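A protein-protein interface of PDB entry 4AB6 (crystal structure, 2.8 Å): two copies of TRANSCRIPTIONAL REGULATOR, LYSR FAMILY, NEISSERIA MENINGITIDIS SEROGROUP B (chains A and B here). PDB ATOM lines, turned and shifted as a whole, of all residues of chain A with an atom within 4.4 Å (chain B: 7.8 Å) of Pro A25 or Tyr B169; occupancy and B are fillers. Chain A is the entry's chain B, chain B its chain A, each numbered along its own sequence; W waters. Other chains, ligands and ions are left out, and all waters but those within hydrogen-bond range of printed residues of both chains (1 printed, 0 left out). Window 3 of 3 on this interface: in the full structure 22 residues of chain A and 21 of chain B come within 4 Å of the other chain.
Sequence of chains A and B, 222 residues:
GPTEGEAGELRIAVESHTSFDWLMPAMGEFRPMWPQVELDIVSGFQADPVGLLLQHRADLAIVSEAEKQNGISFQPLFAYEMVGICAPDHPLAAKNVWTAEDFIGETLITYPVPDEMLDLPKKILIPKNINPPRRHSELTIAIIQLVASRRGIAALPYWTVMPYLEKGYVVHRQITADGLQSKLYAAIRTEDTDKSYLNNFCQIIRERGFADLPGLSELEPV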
ATOM      1  N   ASP A  21      17.818  22.831 -12.397  1.00  0.00           N
ATOM      2  CA  ASP A  21      18.366  21.466 -12.441  1.00  0.00           C
ATOM      3  C   ASP A  21      19.724  21.413 -13.121  1.00  0.00           C
ATOM      4  O   ASP A  21      20.622  20.728 -12.636  1.00  0.00           O
ATOM      5  CB  ASP A  21      17.388  20.492 -13.123  1.00  0.00           C
ATOM      6  CG  ASP A  21      16.144  20.120 -12.328  1.00  0.00           C
ATOM      7  OD1 ASP A  21      15.884  20.762 -11.280  1.00  0.00           O
ATOM      8  OD2 ASP A  21      15.416  19.199 -12.764  1.00  0.00           O
ATOM      9  N   TRP A  22      19.876  22.161 -14.225  1.00  0.00           N
ATOM     10  CA  TRP A  22      21.117  22.245 -14.989  1.00  0.00           C
ATOM     11  C   TRP A  22      21.911  23.534 -14.724  1.00  0.00           C
ATOM     12  O   TRP A  22      23.123  23.558 -14.966  1.00  0.00           O
ATOM     13  CB  TRP A  22      20.874  22.012 -16.491  1.00  0.00           C
ATOM     14  CG  TRP A  22      19.832  22.897 -17.105  1.00  0.00           C
ATOM     15  CD1 TRP A  22      18.543  22.563 -17.395  1.00  0.00           C
ATOM     16  CD2 TRP A  22      20.008  24.254 -17.543  1.00  0.00           C
ATOM     17  NE1 TRP A  22      17.904  23.623 -17.994  1.00  0.00           N
ATOM     18  CE2 TRP A  22      18.779  24.675 -18.096  1.00  0.00           C
ATOM     19  CE3 TRP A  22      21.091  25.152 -17.537  1.00  0.00           C
ATOM     20  CZ2 TRP A  22      18.596  25.963 -18.612  1.00  0.00           C
ATOM     21  CZ3 TRP A  22      20.904  26.429 -18.034  1.00  0.00           C
ATOM     22  CH2 TRP A  22      19.673  26.822 -18.578  1.00  0.00           C
ATOM     23  N   LEU A  23      21.239  24.592 -14.225  1.00  0.00           N
ATOM     24  CA  LEU A  23      21.859  25.887 -13.918  1.00  0.00           C
ATOM     25  C   LEU A  23      22.728  25.834 -12.658  1.00  0.00           C
ATOM     26  O   LEU A  23      23.713  26.566 -12.570  1.00  0.00           O
ATOM     27  CB  LEU A  23      20.785  26.985 -13.799  1.00  0.00           C
ATOM     28  CG  LEU A  23      21.231  28.451 -13.927  1.00  0.00           C
ATOM     29  CD1 LEU A  23      21.778  28.771 -15.325  1.00  0.00           C
ATOM     30  CD2 LEU A  23      20.084  29.383 -13.607  1.00  0.00           C
ATOM     31  N   MET A  24      22.365  24.977 -11.695  1.00  0.00           N
ATOM     32  CA  MET A  24      23.116  24.807 -10.453  1.00  0.00           C
ATOM     33  C   MET A  24      24.505  24.161 -10.662  1.00  0.00           C
ATOM     34  O   MET A  24      25.480  24.761 -10.206  1.00  0.00           O
ATOM     35  CB  MET A  24      22.283  24.075  -9.383  1.00  0.00           C
ATOM     36  CG  MET A  24      21.195  24.928  -8.724  1.00  0.00           C
ATOM     37  SD  MET A  24      21.033  26.661  -9.228  1.00  0.00           S
ATOM     38  CE  MET A  24      21.027  27.417  -7.774  1.00  0.00           C
ATOM     39  N   PRO A  25      24.664  23.009 -11.390  1.00  0.00           N
ATOM     40  CA  PRO A  25      26.022  22.474 -11.607  1.00  0.00           C
ATOM     41  C   PRO A  25      26.900  23.377 -12.483  1.00  0.00           C
ATOM     42  O   PRO A  25      28.125  23.339 -12.340  1.00  0.00           O
ATOM     43  CB  PRO A  25      25.774  21.118 -12.274  1.00  0.00           C
ATOM     44  CG  PRO A  25      24.326  20.820 -12.046  1.00  0.00           C
ATOM     45  CD  PRO A  25      23.657  22.135 -12.028  1.00  0.00           C
ATOM     46  N   ALA A  26      26.276  24.203 -13.364  1.00  0.00           N
ATOM     47  CA  ALA A  26      26.973  25.160 -14.230  1.00  0.00           C
ATOM     48  C   ALA A  26      27.637  26.252 -13.377  1.00  0.00           C
ATOM     49  O   ALA A  26      28.778  26.636 -13.652  1.00  0.00           O
ATOM     50  CB  ALA A  26      26.003  25.773 -15.232  1.00  0.00           C
ATOM     51  N   MET A  27      26.935  26.712 -12.316  1.00  0.00           N
ATOM     52  CA  MET A  27      27.441  27.699 -11.352  1.00  0.00           C
ATOM     53  C   MET A  27      28.608  27.092 -10.567  1.00  0.00           C
ATOM     54  O   MET A  27      29.590  27.784 -10.284  1.00  0.00           O
ATOM     55  CB  MET A  27      26.338  28.142 -10.389  1.00  0.00           C
ATOM     56  CG  MET A  27      25.561  29.324 -10.881  1.00  0.00           C
ATOM     57  SD  MET A  27      24.259  29.753  -9.714  1.00  0.00           S
ATOM     58  CE  MET A  27      22.900  29.235 -10.611  1.00  0.00           C
ATOM     59  N   GLY A  28      28.491  25.802 -10.249  1.00  0.00           N
ATOM     60  CA  GLY A  28      29.520  25.039  -9.559  1.00  0.00           C
ATOM     61  C   GLY A  28      30.796  24.928 -10.364  1.00  0.00           C
ATOM     62  O   GLY A  28      31.889  24.989  -9.799  1.00  0.00           O
ATOM     63  N   GLU A  29      30.663  24.809 -11.699  1.00  0.00           N
ATOM     64  CA  GLU A  29      31.790  24.734 -12.630  1.00  0.00           C
ATOM     65  C   GLU A  29      32.417  26.121 -12.841  1.00  0.00           C
ATOM     66  O   GLU A  29      33.643  26.225 -12.900  1.00  0.00           O
ATOM     67  CB  GLU A  29      31.337  24.137 -13.970  1.00  0.00           C
ATOM     68  CG  GLU A  29      32.471  23.538 -14.784  1.00  0.00           C
ATOM     69  CD  GLU A  29      32.109  22.952 -16.136  1.00  0.00           C
ATOM     70  OE1 GLU A  29      31.027  22.333 -16.252  1.00  0.00           O
ATOM     71  OE2 GLU A  29      32.930  23.074 -17.072  1.00  0.00           O
ATOM     72  N   ARG A 208      27.560  21.445 -20.628  1.00  0.00           N
ATOM     73  CA  ARG A 208      26.870  20.621 -19.632  1.00  0.00           C
ATOM     74  C   ARG A 208      25.528  20.063 -20.109  1.00  0.00           C
ATOM     75  O   ARG A 208      25.268  18.878 -19.908  1.00  0.00           O
ATOM     76  CB  ARG A 208      26.692  21.376 -18.311  1.00  0.00           C
ATOM     77  CG  ARG A 208      27.946  21.446 -17.464  1.00  0.00           C
ATOM     78  CD  ARG A 208      27.606  21.801 -16.035  1.00  0.00           C
ATOM     79  NE  ARG A 208      28.578  21.240 -15.096  1.00  0.00           N
ATOM     80  CZ  ARG A 208      28.450  20.057 -14.500  1.00  0.00           C
ATOM     81  NH1 ARG A 208      27.383  19.298 -14.733  1.00  0.00           N
ATOM     82  NH2 ARG A 208      29.384  19.626 -13.660  1.00  0.00           N
ATOM     83  N   ILE B  85      25.734  25.349   6.634  1.00  0.00           N
ATOM     84  CA  ILE B  85      26.471  25.326   5.371  1.00  0.00           C
ATOM     85  C   ILE B  85      26.966  26.693   4.908  1.00  0.00           C
ATOM     86  O   ILE B  85      26.231  27.680   4.971  1.00  0.00           O
ATOM     87  CB  ILE B  85      25.772  24.503   4.253  1.00  0.00           C
ATOM     88  CG1 ILE B  85      24.314  24.954   4.019  1.00  0.00           C
ATOM     89  CG2 ILE B  85      25.869  23.002   4.541  1.00  0.00           C
ATOM     90  CD1 ILE B  85      23.816  24.771   2.623  1.00  0.00           C
ATOM     91  N   CYS B  86      28.244  26.741   4.474  1.00  0.00           N
ATOM     92  CA  CYS B  86      28.906  27.938   3.959  1.00  0.00           C
ATOM     93  C   CYS B  86      29.849  27.542   2.828  1.00  0.00           C
ATOM     94  O   CYS B  86      30.200  26.369   2.706  1.00  0.00           O
ATOM     95  CB  CYS B  86      29.636  28.699   5.064  1.00  0.00           C
ATOM     96  SG  CYS B  86      31.103  27.861   5.715  1.00  0.00           S
ATOM     97  N   ALA B  87      30.238  28.517   1.993  1.00  0.00           N
ATOM     98  CA  ALA B  87      31.167  28.308   0.880  1.00  0.00           C
ATOM     99  C   ALA B  87      32.542  27.941   1.460  1.00  0.00           C
ATOM    100  O   ALA B  87      32.836  28.362   2.583  1.00  0.00           O
ATOM    101  CB  ALA B  87      31.269  29.578   0.052  1.00  0.00           C
ATOM    102  N   PRO B  88      33.402  27.142   0.774  1.00  0.00           N
ATOM    103  CA  PRO B  88      34.710  26.806   1.374  1.00  0.00           C
ATOM    104  C   PRO B  88      35.551  28.037   1.732  1.00  0.00           C
ATOM    105  O   PRO B  88      36.247  28.024   2.747  1.00  0.00           O
ATOM    106  CB  PRO B  88      35.384  25.936   0.308  1.00  0.00           C
ATOM    107  CG  PRO B  88      34.261  25.411  -0.529  1.00  0.00           C
ATOM    108  CD  PRO B  88      33.250  26.515  -0.555  1.00  0.00           C
ATOM    109  N   ASP B  89      35.409  29.115   0.920  1.00  0.00           N
ATOM    110  CA  ASP B  89      36.091  30.405   1.057  1.00  0.00           C
ATOM    111  C   ASP B  89      35.330  31.454   1.905  1.00  0.00           C
ATOM    112  O   ASP B  89      35.544  32.659   1.750  1.00  0.00           O
ATOM    113  CB  ASP B  89      36.505  30.952  -0.332  1.00  0.00           C
ATOM    114  CG  ASP B  89      35.376  31.407  -1.244  1.00  0.00           C
ATOM    115  OD1 ASP B  89      34.315  30.739  -1.265  1.00  0.00           O
ATOM    116  OD2 ASP B  89      35.568  32.408  -1.969  1.00  0.00           O
ATOM    117  N   ILE B 141      18.410  22.957  -4.205  1.00  0.00           N
ATOM    118  CA  ILE B 141      19.302  23.070  -5.353  1.00  0.00           C
ATOM    119  C   ILE B 141      19.771  24.531  -5.472  1.00  0.00           C
ATOM    120  O   ILE B 141      20.962  24.784  -5.636  1.00  0.00           O
ATOM    121  CB  ILE B 141      18.637  22.607  -6.687  1.00  0.00           C
ATOM    122  CG1 ILE B 141      17.169  22.067  -6.636  1.00  0.00           C
ATOM    123  CG2 ILE B 141      19.578  21.776  -7.532  1.00  0.00           C
ATOM    124  CD1 ILE B 141      16.938  20.579  -6.124  1.00  0.00           C
ATOM    125  N   ILE B 144      21.864  25.797  -2.105  1.00  0.00           N
ATOM    126  CA  ILE B 144      23.258  25.361  -2.223  1.00  0.00           C
ATOM    127  C   ILE B 144      24.108  26.308  -3.082  1.00  0.00           C
ATOM    128  O   ILE B 144      25.226  26.620  -2.674  1.00  0.00           O
ATOM    129  CB  ILE B 144      23.387  23.837  -2.588  1.00  0.00           C
ATOM    130  CG1 ILE B 144      23.396  22.968  -1.318  1.00  0.00           C
ATOM    131  CG2 ILE B 144      24.635  23.518  -3.418  1.00  0.00           C
ATOM    132  CD1 ILE B 144      22.082  22.551  -0.818  1.00  0.00           C
ATOM    133  N   GLN B 145      23.589  26.789  -4.232  1.00  0.00           N
ATOM    134  CA  GLN B 145      24.389  27.681  -5.079  1.00  0.00           C
ATOM    135  C   GLN B 145      24.440  29.114  -4.586  1.00  0.00           C
ATOM    136  O   GLN B 145      25.425  29.801  -4.844  1.00  0.00           O
ATOM    137  CB  GLN B 145      24.077  27.573  -6.573  1.00  0.00           C
ATOM    138  CG  GLN B 145      24.173  26.156  -7.149  1.00  0.00           C
ATOM    139  CD  GLN B 145      25.532  25.500  -7.152  1.00  0.00           C
ATOM    140  OE1 GLN B 145      26.552  26.095  -7.520  1.00  0.00           O
ATOM    141  NE2 GLN B 145      25.545  24.214  -6.834  1.00  0.00           N
ATOM    142  N   VAL B 147      24.564  29.837  -1.321  1.00  0.00           N
ATOM    143  CA  VAL B 147      25.541  29.660  -0.246  1.00  0.00           C
ATOM    144  C   VAL B 147      26.965  29.579  -0.830  1.00  0.00           C
ATOM    145  O   VAL B 147      27.846  30.315  -0.377  1.00  0.00           O
ATOM    146  CB  VAL B 147      25.175  28.450   0.657  1.00  0.00           C
ATOM    147  CG1 VAL B 147      26.274  28.150   1.657  1.00  0.00           C
ATOM    148  CG2 VAL B 147      23.851  28.683   1.386  1.00  0.00           C
ATOM    149  N   ALA B 148      27.159  28.737  -1.872  1.00  0.00           N
ATOM    150  CA  ALA B 148      28.428  28.527  -2.584  1.00  0.00           C
ATOM    151  C   ALA B 148      28.973  29.816  -3.213  1.00  0.00           C
ATOM    152  O   ALA B 148      30.188  29.998  -3.260  1.00  0.00           O
ATOM    153  CB  ALA B 148      28.257  27.459  -3.655  1.00  0.00           C
ATOM    154  N   SER B 149      28.072  30.716  -3.655  1.00  0.00           N
ATOM    155  CA  SER B 149      28.401  31.999  -4.282  1.00  0.00           C
ATOM    156  C   SER B 149      28.604  33.143  -3.266  1.00  0.00           C
ATOM    157  O   SER B 149      28.720  34.311  -3.659  1.00  0.00           O
ATOM    158  CB  SER B 149      27.322  32.372  -5.293  1.00  0.00           C
ATOM    159  OG  SER B 149      27.165  31.342  -6.260  1.00  0.00           O
ATOM    160  N   ARG B 150      28.678  32.789  -1.962  1.00  0.00           N
ATOM    161  CA  ARG B 150      28.850  33.696  -0.821  1.00  0.00           C
ATOM    162  C   ARG B 150      27.715  34.733  -0.670  1.00  0.00           C
ATOM    163  O   ARG B 150      27.959  35.881  -0.292  1.00  0.00           O
ATOM    164  CB  ARG B 150      30.251  34.337  -0.808  1.00  0.00           C
ATOM    165  CG  ARG B 150      31.386  33.359  -0.524  1.00  0.00           C
ATOM    166  CD  ARG B 150      32.740  34.005  -0.296  1.00  0.00           C
ATOM    167  NE  ARG B 150      32.686  35.254   0.463  1.00  0.00           N
ATOM    168  CZ  ARG B 150      33.614  36.214   0.401  1.00  0.00           C
ATOM    169  NH1 ARG B 150      34.676  36.072  -0.387  1.00  0.00           N
ATOM    170  NH2 ARG B 150      33.480  37.323   1.117  1.00  0.00           N
ATOM    171  N   VAL B 161      22.228  17.774   2.417  1.00  0.00           N
ATOM    172  CA  VAL B 161      23.502  18.420   2.130  1.00  0.00           C
ATOM    173  C   VAL B 161      24.510  17.422   1.552  1.00  0.00           C
ATOM    174  O   VAL B 161      25.226  17.758   0.610  1.00  0.00           O
ATOM    175  CB  VAL B 161      23.996  19.141   3.417  1.00  0.00           C
ATOM    176  CG1 VAL B 161      25.470  19.486   3.373  1.00  0.00           C
ATOM    177  CG2 VAL B 161      23.175  20.395   3.683  1.00  0.00           C
ATOM    178  N   PRO B 163      24.987  14.994  -0.791  1.00  0.00           N
ATOM    179  CA  PRO B 163      25.490  14.926  -2.177  1.00  0.00           C
ATOM    180  C   PRO B 163      26.214  16.171  -2.688  1.00  0.00           C
ATOM    181  O   PRO B 163      26.977  16.064  -3.645  1.00  0.00           O
ATOM    182  CB  PRO B 163      24.226  14.659  -3.013  1.00  0.00           C
ATOM    183  CG  PRO B 163      23.190  14.245  -2.045  1.00  0.00           C
ATOM    184  CD  PRO B 163      23.513  14.966  -0.786  1.00  0.00           C
ATOM    185  N   TYR B 164      25.979  17.334  -2.064  1.00  0.00           N
ATOM    186  CA  TYR B 164      26.608  18.599  -2.451  1.00  0.00           C
ATOM    187  C   TYR B 164      27.985  18.790  -1.812  1.00  0.00           C
ATOM    188  O   TYR B 164      28.755  19.645  -2.257  1.00  0.00           O
ATOM    189  CB  TYR B 164      25.691  19.786  -2.135  1.00  0.00           C
ATOM    190  CG  TYR B 164      24.300  19.653  -2.707  1.00  0.00           C
ATOM    191  CD1 TYR B 164      24.045  19.942  -4.043  1.00  0.00           C
ATOM    192  CD2 TYR B 164      23.236  19.236  -1.915  1.00  0.00           C
ATOM    193  CE1 TYR B 164      22.763  19.825  -4.578  1.00  0.00           C
ATOM    194  CE2 TYR B 164      21.949  19.116  -2.438  1.00  0.00           C
ATOM    195  CZ  TYR B 164      21.719  19.408  -3.774  1.00  0.00           C
ATOM    196  OH  TYR B 164      20.460  19.294  -4.306  1.00  0.00           O
ATOM    197  N   LEU B 165      28.301  17.991  -0.781  1.00  0.00           N
ATOM    198  CA  LEU B 165      29.583  18.036  -0.072  1.00  0.00           C
ATOM    199  C   LEU B 165      30.649  17.361  -0.889  1.00  0.00           C
ATOM    200  O   LEU B 165      31.820  17.739  -0.820  1.00  0.00           O
ATOM    201  CB  LEU B 165      29.485  17.335   1.288  1.00  0.00           C
ATOM    202  CG  LEU B 165      28.590  17.976   2.333  1.00  0.00           C
ATOM    203  CD1 LEU B 165      28.376  17.034   3.490  1.00  0.00           C
ATOM    204  CD2 LEU B 165      29.144  19.330   2.794  1.00  0.00           C
ATOM    205  N   GLU B 166      30.208  16.351  -1.668  1.00  0.00           N
ATOM    206  CA  GLU B 166      30.981  15.485  -2.557  1.00  0.00           C
ATOM    207  C   GLU B 166      31.417  16.194  -3.859  1.00  0.00           C
ATOM    208  O   GLU B 166      32.207  15.636  -4.613  1.00  0.00           O
ATOM    209  CB  GLU B 166      30.159  14.220  -2.884  1.00  0.00           C
ATOM    210  CG  GLU B 166      29.672  13.445  -1.666  1.00  0.00           C
ATOM    211  CD  GLU B 166      28.751  12.262  -1.922  1.00  0.00           C
ATOM    212  OE1 GLU B 166      28.253  12.116  -3.063  1.00  0.00           O
ATOM    213  OE2 GLU B 166      28.519  11.483  -0.967  1.00  0.00           O
ATOM    214  N   LYS B 167      30.905  17.412  -4.106  1.00  0.00           N
ATOM    215  CA  LYS B 167      31.162  18.266  -5.268  1.00  0.00           C
ATOM    216  C   LYS B 167      31.971  19.541  -4.952  1.00  0.00           C
ATOM    217  O   LYS B 167      32.373  20.254  -5.879  1.00  0.00           O
ATOM    218  CB  LYS B 167      29.837  18.580  -5.982  1.00  0.00           C
ATOM    219  CG  LYS B 167      29.199  17.334  -6.581  1.00  0.00           C
ATOM    220  CD  LYS B 167      28.020  17.648  -7.486  1.00  0.00           C
ATOM    221  CE  LYS B 167      27.609  16.453  -8.317  1.00  0.00           C
ATOM    222  NZ  LYS B 167      26.779  15.440  -7.596  1.00  0.00           N
ATOM    223  N   GLY B 168      32.227  19.786  -3.661  1.00  0.00           N
ATOM    224  CA  GLY B 168      33.011  20.917  -3.176  1.00  0.00           C
ATOM    225  C   GLY B 168      32.335  22.266  -3.256  1.00  0.00           C
ATOM    226  O   GLY B 168      33.021  23.292  -3.195  1.00  0.00           O
ATOM    227  N   TYR B 169      30.998  22.295  -3.375  1.00  0.00           N
ATOM    228  CA  TYR B 169      30.226  23.539  -3.446  1.00  0.00           C
ATOM    229  C   TYR B 169      30.191  24.235  -2.091  1.00  0.00           C
ATOM    230  O   TYR B 169      30.423  25.443  -2.003  1.00  0.00           O
ATOM    231  CB  TYR B 169      28.774  23.279  -3.885  1.00  0.00           C
ATOM    232  CG  TYR B 169      28.559  22.593  -5.219  1.00  0.00           C
ATOM    233  CD1 TYR B 169      29.351  22.907  -6.324  1.00  0.00           C
ATOM    234  CD2 TYR B 169      27.484  21.735  -5.417  1.00  0.00           C
ATOM    235  CE1 TYR B 169      29.124  22.310  -7.566  1.00  0.00           C
ATOM    236  CE2 TYR B 169      27.241  21.142  -6.656  1.00  0.00           C
ATOM    237  CZ  TYR B 169      28.059  21.438  -7.728  1.00  0.00           C
ATOM    238  OH  TYR B 169      27.798  20.861  -8.940  1.00  0.00           O
ATOM    239  N   VAL B 170      29.845  23.473  -1.036  1.00  0.00           N
ATOM    240  CA  VAL B 170      29.698  23.965   0.330  1.00  0.00           C
ATOM    241  C   VAL B 170      30.396  23.061   1.349  1.00  0.00           C
ATOM    242  O   VAL B 170      30.659  21.891   1.065  1.00  0.00           O
ATOM    243  CB  VAL B 170      28.201  24.166   0.701  1.00  0.00           C
ATOM    244  CG1 VAL B 170      27.567  25.280  -0.122  1.00  0.00           C
ATOM    245  CG2 VAL B 170      27.400  22.869   0.569  1.00  0.00           C
ATOM    246  N   VAL B 171      30.666  23.608   2.542  1.00  0.00           N
ATOM    247  CA  VAL B 171      31.242  22.860   3.657  1.00  0.00           C
ATOM    248  C   VAL B 171      30.197  22.783   4.768  1.00  0.00           C
ATOM    249  O   VAL B 171      29.515  23.775   5.019  1.00  0.00           O
ATOM    250  CB  VAL B 171      32.652  23.348   4.139  1.00  0.00           C
ATOM    251  CG1 VAL B 171      33.716  23.103   3.074  1.00  0.00           C
ATOM    252  CG2 VAL B 171      32.653  24.812   4.578  1.00  0.00           C
HETATM  253  O   HOH W   1      29.681  21.752 -10.731  1.00  0.00           O
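OE1 of Gln B145 lies within hydrogen-bond range of N of Gly A28 (3.4 Å).
The side-chain amide oxygen (OE1) of Gln B145 sits close to the backbone carbonyl oxygen (O) of Met A24 (3.2 Å).
The backbone carbonyl oxygen of Pro A25 lies within hydrogen-bond range of the guanidinium group of Arg A208.
The backbone carbonyl oxygen (O) of Gln B145 lies within hydrogen-bond range of the side-chain hydroxyl (OG) of Ser B149, 2.7 Å away.
Met A24 touches Ile B141.
Pro A25 touches Tyr B169.
Met A27 touches Gln B145.
Tyr B169 touches Gly A28 (CE1 to CA, 3.4 Å).
Pro A25 touches just one residue of chain B: Tyr B169.
Tyr B169 touches just these residues of chain A: Pro A25 and Gly A28.
Of the printed residues of chain B, Gly A28 touches Gln B145 (3.4 Å) and Tyr B169 (3.4 Å).
Printed residues of chain B within 4 Å of Met A24: Ile B141 (3.1 Å) and Gln B145 (3.1 Å).
The nearest residue of chain B that does not touch Pro A25 is Gln B145 (4.8 Å).
Hydrophobic or aromatic side chains of chain B within 4 Å of the printed part of chain A: Ile B141 and Tyr B169.
Of the 10 printed residues of chain A, 4 touch a printed residue of chain B.
Printed residues of chain A that touch a printed residue of chain B: Met A24, Pro A25, Met A27 and Gly A28.
Hydrophobic or aromatic side chains of chain A within 4 Å of the printed part of chain B: Met A24, Pro A25 and Met A27.
Along chain A the printed residues that touch a printed residue of chain B span positions 24 to 28.
No position is printed for both chains.
Water W1 lies within hydrogen-bond range of O of Pro A25 (2.7 Å), OH of Tyr B169 (2.7 Å) and N of Glu A29 (3.4 Å).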
